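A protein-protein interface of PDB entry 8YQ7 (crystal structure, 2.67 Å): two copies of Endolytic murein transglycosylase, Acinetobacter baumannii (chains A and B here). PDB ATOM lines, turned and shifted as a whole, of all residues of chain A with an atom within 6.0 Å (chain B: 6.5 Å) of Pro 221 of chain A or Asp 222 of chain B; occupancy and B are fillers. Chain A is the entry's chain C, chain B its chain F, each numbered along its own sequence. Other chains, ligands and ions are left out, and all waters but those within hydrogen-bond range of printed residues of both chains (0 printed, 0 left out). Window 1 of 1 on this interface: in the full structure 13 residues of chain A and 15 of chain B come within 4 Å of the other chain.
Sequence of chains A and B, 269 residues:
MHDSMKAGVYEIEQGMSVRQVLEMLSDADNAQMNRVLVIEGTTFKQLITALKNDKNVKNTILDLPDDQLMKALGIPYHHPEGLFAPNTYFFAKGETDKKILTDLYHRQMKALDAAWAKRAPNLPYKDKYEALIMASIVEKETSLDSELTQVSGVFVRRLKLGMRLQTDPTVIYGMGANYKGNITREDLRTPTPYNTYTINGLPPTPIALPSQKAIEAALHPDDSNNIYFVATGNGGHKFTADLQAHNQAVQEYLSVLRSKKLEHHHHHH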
ATOM      1  N   ALA A 120      -8.922 -16.439 -14.655  1.00  0.00           N
ATOM      2  CA  ALA A 120      -9.022 -16.659 -13.226  1.00  0.00           C
ATOM      3  C   ALA A 120     -10.462 -16.955 -12.844  1.00  0.00           C
ATOM      4  O   ALA A 120     -11.392 -16.606 -13.571  1.00  0.00           O
ATOM      5  CB  ALA A 120      -8.519 -15.439 -12.473  1.00  0.00           C
ATOM      6  N   LEU A 123     -14.762 -14.551 -11.942  1.00  0.00           N
ATOM      7  CA  LEU A 123     -14.787 -13.263 -12.622  1.00  0.00           C
ATOM      8  C   LEU A 123     -16.224 -12.879 -12.957  1.00  0.00           C
ATOM      9  O   LEU A 123     -17.053 -13.749 -13.238  1.00  0.00           O
ATOM     10  CB  LEU A 123     -13.963 -13.315 -13.905  1.00  0.00           C
ATOM     11  CG  LEU A 123     -12.454 -13.300 -13.661  1.00  0.00           C
ATOM     12  CD1 LEU A 123     -11.700 -13.558 -14.956  1.00  0.00           C
ATOM     13  CD2 LEU A 123     -11.978 -12.011 -13.055  1.00  0.00           C
ATOM     14  N   THR A 149      -3.017  -4.943 -14.146  1.00  0.00           N
ATOM     15  CA  THR A 149      -3.729  -5.824 -13.226  1.00  0.00           C
ATOM     16  C   THR A 149      -4.442  -5.030 -12.146  1.00  0.00           C
ATOM     17  O   THR A 149      -5.543  -5.397 -11.716  1.00  0.00           O
ATOM     18  CB  THR A 149      -2.762  -6.824 -12.596  1.00  0.00           C
ATOM     19  OG1 THR A 149      -1.573  -6.146 -12.169  1.00  0.00           O
ATOM     20  CG2 THR A 149      -2.408  -7.887 -13.617  1.00  0.00           C
ATOM     21  N   SER A 152      -7.585  -3.184 -13.630  1.00  0.00           N
ATOM     22  CA  SER A 152      -8.625  -4.176 -13.843  1.00  0.00           C
ATOM     23  C   SER A 152      -9.237  -4.571 -12.514  1.00  0.00           C
ATOM     24  O   SER A 152     -10.466  -4.594 -12.367  1.00  0.00           O
ATOM     25  CB  SER A 152      -8.052  -5.388 -14.591  1.00  0.00           C
ATOM     26  OG  SER A 152      -7.526  -6.360 -13.717  1.00  0.00           O
ATOM     27  N   GLY A 153      -8.393  -4.816 -11.507  1.00  0.00           N
ATOM     28  CA  GLY A 153      -8.928  -5.167 -10.203  1.00  0.00           C
ATOM     29  C   GLY A 153      -9.945  -4.149  -9.729  1.00  0.00           C
ATOM     30  O   GLY A 153     -11.099  -4.490  -9.446  1.00  0.00           O
ATOM     31  N   VAL A 156     -12.981  -4.596 -11.739  1.00  0.00           N
ATOM     32  CA  VAL A 156     -13.612  -5.891 -11.511  1.00  0.00           C
ATOM     33  C   VAL A 156     -14.332  -5.883 -10.177  1.00  0.00           C
ATOM     34  O   VAL A 156     -15.522  -6.202 -10.091  1.00  0.00           O
ATOM     35  CB  VAL A 156     -12.574  -7.024 -11.583  1.00  0.00           C
ATOM     36  CG1 VAL A 156     -13.101  -8.251 -10.878  1.00  0.00           C
ATOM     37  CG2 VAL A 156     -12.247  -7.354 -13.027  1.00  0.00           C
ATOM     38  N   ARG A 157     -13.619  -5.504  -9.117  1.00  0.00           N
ATOM     39  CA  ARG A 157     -14.242  -5.442  -7.801  1.00  0.00           C
ATOM     40  C   ARG A 157     -15.487  -4.562  -7.841  1.00  0.00           C
ATOM     41  O   ARG A 157     -16.544  -4.937  -7.316  1.00  0.00           O
ATOM     42  CB  ARG A 157     -13.225  -4.942  -6.771  1.00  0.00           C
ATOM     43  CG  ARG A 157     -12.228  -6.042  -6.307  1.00  0.00           C
ATOM     44  CD  ARG A 157     -11.209  -5.510  -5.291  1.00  0.00           C
ATOM     45  NE  ARG A 157     -10.141  -4.683  -5.846  1.00  0.00           N
ATOM     46  CZ  ARG A 157      -9.045  -5.159  -6.412  1.00  0.00           C
ATOM     47  NH1 ARG A 157      -8.869  -6.473  -6.491  1.00  0.00           N
ATOM     48  NH2 ARG A 157      -8.120  -4.336  -6.886  1.00  0.00           N
ATOM     49  N   GLU A 216      -5.376  -9.902 -21.062  1.00  0.00           N
ATOM     50  CA  GLU A 216      -4.886 -10.747 -19.983  1.00  0.00           C
ATOM     51  C   GLU A 216      -5.127 -10.098 -18.631  1.00  0.00           C
ATOM     52  O   GLU A 216      -5.583 -10.765 -17.695  1.00  0.00           O
ATOM     53  CB  GLU A 216      -3.403 -11.053 -20.184  1.00  0.00           C
ATOM     54  CG  GLU A 216      -3.102 -12.000 -21.340  1.00  0.00           C
ATOM     55  CD  GLU A 216      -3.278 -13.463 -20.921  1.00  0.00           C
ATOM     56  OE1 GLU A 216      -2.561 -13.906 -19.983  1.00  0.00           O
ATOM     57  OE2 GLU A 216      -4.146 -14.155 -21.499  1.00  0.00           O
ATOM     58  N   ALA A 217      -4.865  -8.792 -18.519  1.00  0.00           N
ATOM     59  CA  ALA A 217      -5.107  -8.096 -17.255  1.00  0.00           C
ATOM     60  C   ALA A 217      -6.581  -8.146 -16.873  1.00  0.00           C
ATOM     61  O   ALA A 217      -6.928  -8.452 -15.723  1.00  0.00           O
ATOM     62  CB  ALA A 217      -4.632  -6.647 -17.364  1.00  0.00           C
ATOM     63  N   ALA A 218      -7.464  -7.894 -17.842  1.00  0.00           N
ATOM     64  CA  ALA A 218      -8.896  -7.984 -17.599  1.00  0.00           C
ATOM     65  C   ALA A 218      -9.288  -9.337 -17.038  1.00  0.00           C
ATOM     66  O   ALA A 218     -10.237  -9.426 -16.250  1.00  0.00           O
ATOM     67  CB  ALA A 218      -9.660  -7.720 -18.898  1.00  0.00           C
ATOM     68  N   LEU A 219      -8.596 -10.400 -17.443  1.00  0.00           N
ATOM     69  CA  LEU A 219      -8.943 -11.740 -16.977  1.00  0.00           C
ATOM     70  C   LEU A 219      -8.127 -12.196 -15.777  1.00  0.00           C
ATOM     71  O   LEU A 219      -8.318 -13.325 -15.308  1.00  0.00           O
ATOM     72  CB  LEU A 219      -8.802 -12.737 -18.129  1.00  0.00           C
ATOM     73  CG  LEU A 219      -9.802 -12.427 -19.250  1.00  0.00           C
ATOM     74  CD1 LEU A 219      -9.499 -13.109 -20.559  1.00  0.00           C
ATOM     75  CD2 LEU A 219     -11.228 -12.772 -18.778  1.00  0.00           C
ATOM     76  N   HIS A 220      -7.243 -11.352 -15.247  1.00  0.00           N
ATOM     77  CA  HIS A 220      -6.415 -11.716 -14.096  1.00  0.00           C
ATOM     78  C   HIS A 220      -6.267 -10.514 -13.177  1.00  0.00           C
ATOM     79  O   HIS A 220      -5.190  -9.913 -13.071  1.00  0.00           O
ATOM     80  CB  HIS A 220      -5.062 -12.247 -14.570  1.00  0.00           C
ATOM     81  CG  HIS A 220      -5.176 -13.545 -15.302  1.00  0.00           C
ATOM     82  ND1 HIS A 220      -5.162 -13.617 -16.676  1.00  0.00           N
ATOM     83  CD2 HIS A 220      -5.358 -14.810 -14.859  1.00  0.00           C
ATOM     84  CE1 HIS A 220      -5.313 -14.874 -17.050  1.00  0.00           C
ATOM     85  NE2 HIS A 220      -5.431 -15.617 -15.965  1.00  0.00           N
ATOM     86  N   PRO A 221      -7.336 -10.152 -12.470  1.00  0.00           N
ATOM     87  CA  PRO A 221      -7.270  -9.013 -11.544  1.00  0.00           C
ATOM     88  C   PRO A 221      -6.363  -9.303 -10.360  1.00  0.00           C
ATOM     89  O   PRO A 221      -6.113 -10.453  -9.998  1.00  0.00           O
ATOM     90  CB  PRO A 221      -8.725  -8.829 -11.094  1.00  0.00           C
ATOM     91  CG  PRO A 221      -9.366 -10.179 -11.308  1.00  0.00           C
ATOM     92  CD  PRO A 221      -8.676 -10.768 -12.512  1.00  0.00           C
ATOM     93  N   ASP A 222      -5.883  -8.228  -9.741  1.00  0.00           N
ATOM     94  CA  ASP A 222      -4.954  -8.339  -8.625  1.00  0.00           C
ATOM     95  C   ASP A 222      -5.697  -8.640  -7.326  1.00  0.00           C
ATOM     96  O   ASP A 222      -6.912  -8.452  -7.208  1.00  0.00           O
ATOM     97  CB  ASP A 222      -4.131  -7.055  -8.476  1.00  0.00           C
ATOM     98  CG  ASP A 222      -4.887  -5.929  -7.761  1.00  0.00           C
ATOM     99  OD1 ASP A 222      -6.125  -5.766  -7.956  1.00  0.00           O
ATOM    100  OD2 ASP A 222      -4.194  -5.174  -7.029  1.00  0.00           O
ATOM    101  N   ASP A 223      -4.938  -9.091  -6.334  1.00  0.00           N
ATOM    102  CA  ASP A 223      -5.485  -9.469  -5.036  1.00  0.00           C
ATOM    103  C   ASP A 223      -5.365  -8.249  -4.136  1.00  0.00           C
ATOM    104  O   ASP A 223      -4.301  -7.979  -3.572  1.00  0.00           O
ATOM    105  CB  ASP A 223      -4.745 -10.679  -4.480  1.00  0.00           C
ATOM    106  CG  ASP A 223      -5.182 -11.036  -3.080  1.00  0.00           C
ATOM    107  OD1 ASP A 223      -4.307 -11.400  -2.253  1.00  0.00           O
ATOM    108  OD2 ASP A 223      -6.410 -10.962  -2.823  1.00  0.00           O
ATOM    109  N   THR B 149       2.350 -11.945 -12.329  1.00  0.00           N
ATOM    110  CA  THR B 149       1.447 -11.869 -11.181  1.00  0.00           C
ATOM    111  C   THR B 149       0.946 -13.252 -10.778  1.00  0.00           C
ATOM    112  O   THR B 149       0.931 -13.599  -9.587  1.00  0.00           O
ATOM    113  CB  THR B 149       0.283 -10.923 -11.487  1.00  0.00           C
ATOM    114  OG1 THR B 149      -0.200 -11.148 -12.819  1.00  0.00           O
ATOM    115  CG2 THR B 149       0.727  -9.489 -11.344  1.00  0.00           C
ATOM    116  N   GLN B 150       0.583 -14.080 -11.761  1.00  0.00           N
ATOM    117  CA  GLN B 150       0.082 -15.410 -11.434  1.00  0.00           C
ATOM    118  C   GLN B 150       1.141 -16.214 -10.694  1.00  0.00           C
ATOM    119  O   GLN B 150       0.870 -16.814  -9.645  1.00  0.00           O
ATOM    120  CB  GLN B 150      -0.372 -16.122 -12.698  1.00  0.00           C
ATOM    121  CG  GLN B 150      -1.498 -15.383 -13.391  1.00  0.00           C
ATOM    122  CD  GLN B 150      -2.032 -16.137 -14.584  1.00  0.00           C
ATOM    123  OE1 GLN B 150      -1.930 -15.672 -15.724  1.00  0.00           O
ATOM    124  NE2 GLN B 150      -2.621 -17.307 -14.327  1.00  0.00           N
ATOM    125  N   VAL B 151       2.372 -16.196 -11.190  1.00  0.00           N
ATOM    126  CA  VAL B 151       3.423 -16.906 -10.473  1.00  0.00           C
ATOM    127  C   VAL B 151       3.529 -16.342  -9.067  1.00  0.00           C
ATOM    128  O   VAL B 151       3.514 -17.086  -8.076  1.00  0.00           O
ATOM    129  CB  VAL B 151       4.752 -16.842 -11.244  1.00  0.00           C
ATOM    130  CG1 VAL B 151       5.888 -17.325 -10.377  1.00  0.00           C
ATOM    131  CG2 VAL B 151       4.632 -17.718 -12.505  1.00  0.00           C
ATOM    132  N   SER B 152       3.566 -15.008  -8.961  1.00  0.00           N
ATOM    133  CA  SER B 152       3.667 -14.367  -7.655  1.00  0.00           C
ATOM    134  C   SER B 152       2.539 -14.836  -6.749  1.00  0.00           C
ATOM    135  O   SER B 152       2.760 -15.216  -5.586  1.00  0.00           O
ATOM    136  CB  SER B 152       3.645 -12.847  -7.816  1.00  0.00           C
ATOM    137  OG  SER B 152       3.813 -12.213  -6.565  1.00  0.00           O
ATOM    138  N   GLY B 153       1.322 -14.863  -7.289  1.00  0.00           N
ATOM    139  CA  GLY B 153       0.209 -15.348  -6.497  1.00  0.00           C
ATOM    140  C   GLY B 153       0.503 -16.713  -5.919  1.00  0.00           C
ATOM    141  O   GLY B 153       0.467 -16.909  -4.698  1.00  0.00           O
ATOM    142  N   VAL B 154       0.907 -17.651  -6.787  1.00  0.00           N
ATOM    143  CA  VAL B 154       1.166 -19.020  -6.344  1.00  0.00           C
ATOM    144  C   VAL B 154       2.063 -19.006  -5.115  1.00  0.00           C
ATOM    145  O   VAL B 154       1.754 -19.616  -4.086  1.00  0.00           O
ATOM    146  CB  VAL B 154       1.798 -19.846  -7.485  1.00  0.00           C
ATOM    147  CG1 VAL B 154       2.613 -21.009  -6.921  1.00  0.00           C
ATOM    148  CG2 VAL B 154       0.738 -20.372  -8.457  1.00  0.00           C
ATOM    149  N   ARG B 157       0.450 -16.882  -1.908  1.00  0.00           N
ATOM    150  CA  ARG B 157      -0.554 -17.688  -1.224  1.00  0.00           C
ATOM    151  C   ARG B 157       0.103 -18.823  -0.446  1.00  0.00           C
ATOM    152  O   ARG B 157      -0.256 -19.073   0.710  1.00  0.00           O
ATOM    153  CB  ARG B 157      -1.584 -18.237  -2.210  1.00  0.00           C
ATOM    154  CG  ARG B 157      -2.669 -17.228  -2.596  1.00  0.00           C
ATOM    155  CD  ARG B 157      -3.644 -17.838  -3.598  1.00  0.00           C
ATOM    156  NE  ARG B 157      -3.043 -17.944  -4.923  1.00  0.00           N
ATOM    157  CZ  ARG B 157      -2.913 -16.934  -5.776  1.00  0.00           C
ATOM    158  NH1 ARG B 157      -3.347 -15.716  -5.447  1.00  0.00           N
ATOM    159  NH2 ARG B 157      -2.341 -17.145  -6.958  1.00  0.00           N
ATOM    160  N   ALA B 217       5.439  -7.337  -9.603  1.00  0.00           N
ATOM    161  CA  ALA B 217       4.605  -8.528  -9.528  1.00  0.00           C
ATOM    162  C   ALA B 217       4.694  -9.155  -8.147  1.00  0.00           C
ATOM    163  O   ALA B 217       3.670  -9.511  -7.553  1.00  0.00           O
ATOM    164  CB  ALA B 217       5.029  -9.533 -10.601  1.00  0.00           C
ATOM    165  N   HIS B 220       2.421  -7.417  -6.067  1.00  0.00           N
ATOM    166  CA  HIS B 220       1.025  -7.369  -6.506  1.00  0.00           C
ATOM    167  C   HIS B 220       0.564  -8.717  -7.033  1.00  0.00           C
ATOM    168  O   HIS B 220       0.385  -8.900  -8.242  1.00  0.00           O
ATOM    169  CB  HIS B 220       0.834  -6.287  -7.570  1.00  0.00           C
ATOM    170  CG  HIS B 220       1.013  -4.902  -7.043  1.00  0.00           C
ATOM    171  ND1 HIS B 220       2.148  -4.157  -7.286  1.00  0.00           N
ATOM    172  CD2 HIS B 220       0.239  -4.157  -6.218  1.00  0.00           C
ATOM    173  CE1 HIS B 220       2.042  -2.992  -6.672  1.00  0.00           C
ATOM    174  NE2 HIS B 220       0.896  -2.968  -6.016  1.00  0.00           N
ATOM    175  N   PRO B 221       0.341  -9.689  -6.153  1.00  0.00           N
ATOM    176  CA  PRO B 221      -0.114 -11.011  -6.607  1.00  0.00           C
ATOM    177  C   PRO B 221      -1.522 -10.967  -7.186  1.00  0.00           C
ATOM    178  O   PRO B 221      -2.313 -10.072  -6.902  1.00  0.00           O
ATOM    179  CB  PRO B 221      -0.075 -11.864  -5.333  1.00  0.00           C
ATOM    180  CG  PRO B 221      -0.170 -10.875  -4.196  1.00  0.00           C
ATOM    181  CD  PRO B 221       0.537  -9.637  -4.689  1.00  0.00           C
ATOM    182  N   ASP B 222      -1.831 -11.966  -8.011  1.00  0.00           N
ATOM    183  CA  ASP B 222      -3.143 -12.038  -8.637  1.00  0.00           C
ATOM    184  C   ASP B 222      -4.175 -12.593  -7.661  1.00  0.00           C
ATOM    185  O   ASP B 222      -3.847 -13.212  -6.649  1.00  0.00           O
ATOM    186  CB  ASP B 222      -3.118 -12.903  -9.900  1.00  0.00           C
ATOM    187  CG  ASP B 222      -3.041 -14.392  -9.592  1.00  0.00           C
ATOM    188  OD1 ASP B 222      -2.280 -14.740  -8.666  1.00  0.00           O
ATOM    189  OD2 ASP B 222      -3.747 -15.198 -10.262  1.00  0.00           O
ATOM    190  N   ASP B 223      -5.441 -12.367  -7.986  1.00  0.00           N
ATOM    191  CA  ASP B 223      -6.561 -12.790  -7.156  1.00  0.00           C
ATOM    192  C   ASP B 223      -7.054 -14.129  -7.675  1.00  0.00           C
ATOM    193  O   ASP B 223      -7.876 -14.186  -8.593  1.00  0.00           O
ATOM    194  CB  ASP B 223      -7.682 -11.756  -7.183  1.00  0.00           C
ATOM    195  CG  ASP B 223      -8.945 -12.251  -6.492  1.00  0.00           C
ATOM    196  OD1 ASP B 223      -8.834 -12.876  -5.409  1.00  0.00           O
ATOM    197  OD2 ASP B 223     -10.046 -12.039  -7.048  1.00  0.00           O
ATOM    198  N   SER B 224      -6.572 -15.206  -7.067  1.00  0.00           N
ATOM    199  CA  SER B 224      -6.916 -16.550  -7.511  1.00  0.00           C
ATOM    200  C   SER B 224      -6.617 -17.513  -6.376  1.00  0.00           C
ATOM    201  O   SER B 224      -5.982 -17.157  -5.384  1.00  0.00           O
ATOM    202  CB  SER B 224      -6.141 -16.940  -8.769  1.00  0.00           C
ATOM    203  OG  SER B 224      -6.617 -18.164  -9.281  1.00  0.00           O
ATOM    204  N   ASN B 225      -7.056 -18.753  -6.550  1.00  0.00           N
ATOM    205  CA  ASN B 225      -6.764 -19.808  -5.592  1.00  0.00           C
ATOM    206  C   ASN B 225      -5.648 -20.735  -6.051  1.00  0.00           C
ATOM    207  O   ASN B 225      -5.301 -21.664  -5.322  1.00  0.00           O
ATOM    208  CB  ASN B 225      -8.038 -20.607  -5.313  1.00  0.00           C
ATOM    209  CG  ASN B 225      -8.681 -21.132  -6.581  1.00  0.00           C
ATOM    210  OD1 ASN B 225      -8.142 -20.969  -7.685  1.00  0.00           O
ATOM    211  ND2 ASN B 225      -9.847 -21.753  -6.436  1.00  0.00           N
ATOM    212  N   ASN B 226      -5.056 -20.490  -7.215  1.00  0.00           N
ATOM    213  CA  ASN B 226      -4.066 -21.404  -7.762  1.00  0.00           C
ATOM    214  C   ASN B 226      -2.790 -21.387  -6.937  1.00  0.00           C
ATOM    215  O   ASN B 226      -2.241 -20.320  -6.655  1.00  0.00           O
ATOM    216  CB  ASN B 226      -3.752 -21.034  -9.206  1.00  0.00           C
ATOM    217  CG  ASN B 226      -4.910 -21.295 -10.137  1.00  0.00           C
ATOM    218  OD1 ASN B 226      -4.779 -21.153 -11.347  1.00  0.00           O
ATOM    219  ND2 ASN B 226      -6.039 -21.706  -9.586  1.00  0.00           N
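The backbone carbonyl oxygen of Pro 221 of chain A is in hydrogen-bond range of the backbone NH of Asp 223 of chain B (2.9 Å).
O of Pro 221 of chain B is in hydrogen-bond range of N of Asp 223 of chain A (2.9 Å).
The backbone carbonyl oxygen of Thr 149 of chain A sits at hydrogen-bond distance from the backbone NH of Asp 222 of chain A (3.5 Å).
NH2 of Arg 157 of chain A lies within salt-bridge range of OD1 of Asp 222 of chain A, 2.7 Å away.
The backbone carbonyl oxygen of Glu 216 of chain A sits at hydrogen-bond distance from a ring nitrogen (ND1) of His 220 of chain A (3.1 Å).
NH2 of Arg 157 of chain B lies within salt-bridge range of OD1 of Asp 222 of chain B (3.0 Å).
Among the printed residues, pairs that only touch across the chains: His 220 of chain A with Gln 150 of chain B (3.5 Å), Pro 221 of chain A with Asp 222 of chain B (3.6 Å), Asp 222 of chain A with Pro 221 of chain B (3.6 Å), Asp 222 of chain A with Asp 223 of chain B (3.4 Å), Asp 223 of chain A with Asp 222 of chain B (3.5 Å) and Asp 223 of chain A with Asp 223 of chain B (3.7 Å).
Thr 149 of chain A touches none of the printed residues of chain B.
Of the printed residues of chain B, His 220 of chain A touches Gln 150.
Of chain B, only Asp 222 and Asp 223 come within 4 Å of Pro 221 of chain A.
Of the printed residues of chain B, Asp 222 of chain A touches Pro 221 and Asp 223.
Of the printed residues of chain B, Asp 223 of chain A touches Pro 221 (2.9 Å), Asp 222 (3.5 Å) and Asp 223 (3.7 Å).
Of the printed residues of chain A, Gln 150 of chain B touches His 220 (3.5 Å).
Val 154 of chain B touches none of the printed residues of chain A.
Printed residues of chain A within 4 Å of Pro 221 of chain B: Asp 222 (3.6 Å) and Asp 223 (2.9 Å).
Asp 222 of chain B touches two residues of chain A.
The nearest printed residue of chain A that does not touch Asp 223 of chain B is Ala 120 of chain A (4.1 Å).
Of the 15 printed residues of chain B, 4 touch a printed residue of chain A.
Of the 15 printed residues of chain A, 4 touch a printed residue of chain B.
Along chain A the printed residues that touch a printed residue of chain B span positions 220 to 223.
Pro 221 of chain A touches Asp 222 of chain B, and with the chains exchanged Asp 222 of chain A touches Pro 221 of chain B.
Pro 221 of chain A touches Asp 223 of chain B, and with the chains exchanged Asp 223 of chain A touches Pro 221 of chain B.
Asp 222 of chain A touches Asp 223 of chain B, and with the chains exchanged Asp 223 of chain A touches Asp 222 of chain B.
Asp 223 of chain A touches its own counterpart, Asp 223 of chain B.
Of the 8 pairs that touch across the chains among the printed residues, 7 have their exchanged pair printed and touching as well.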
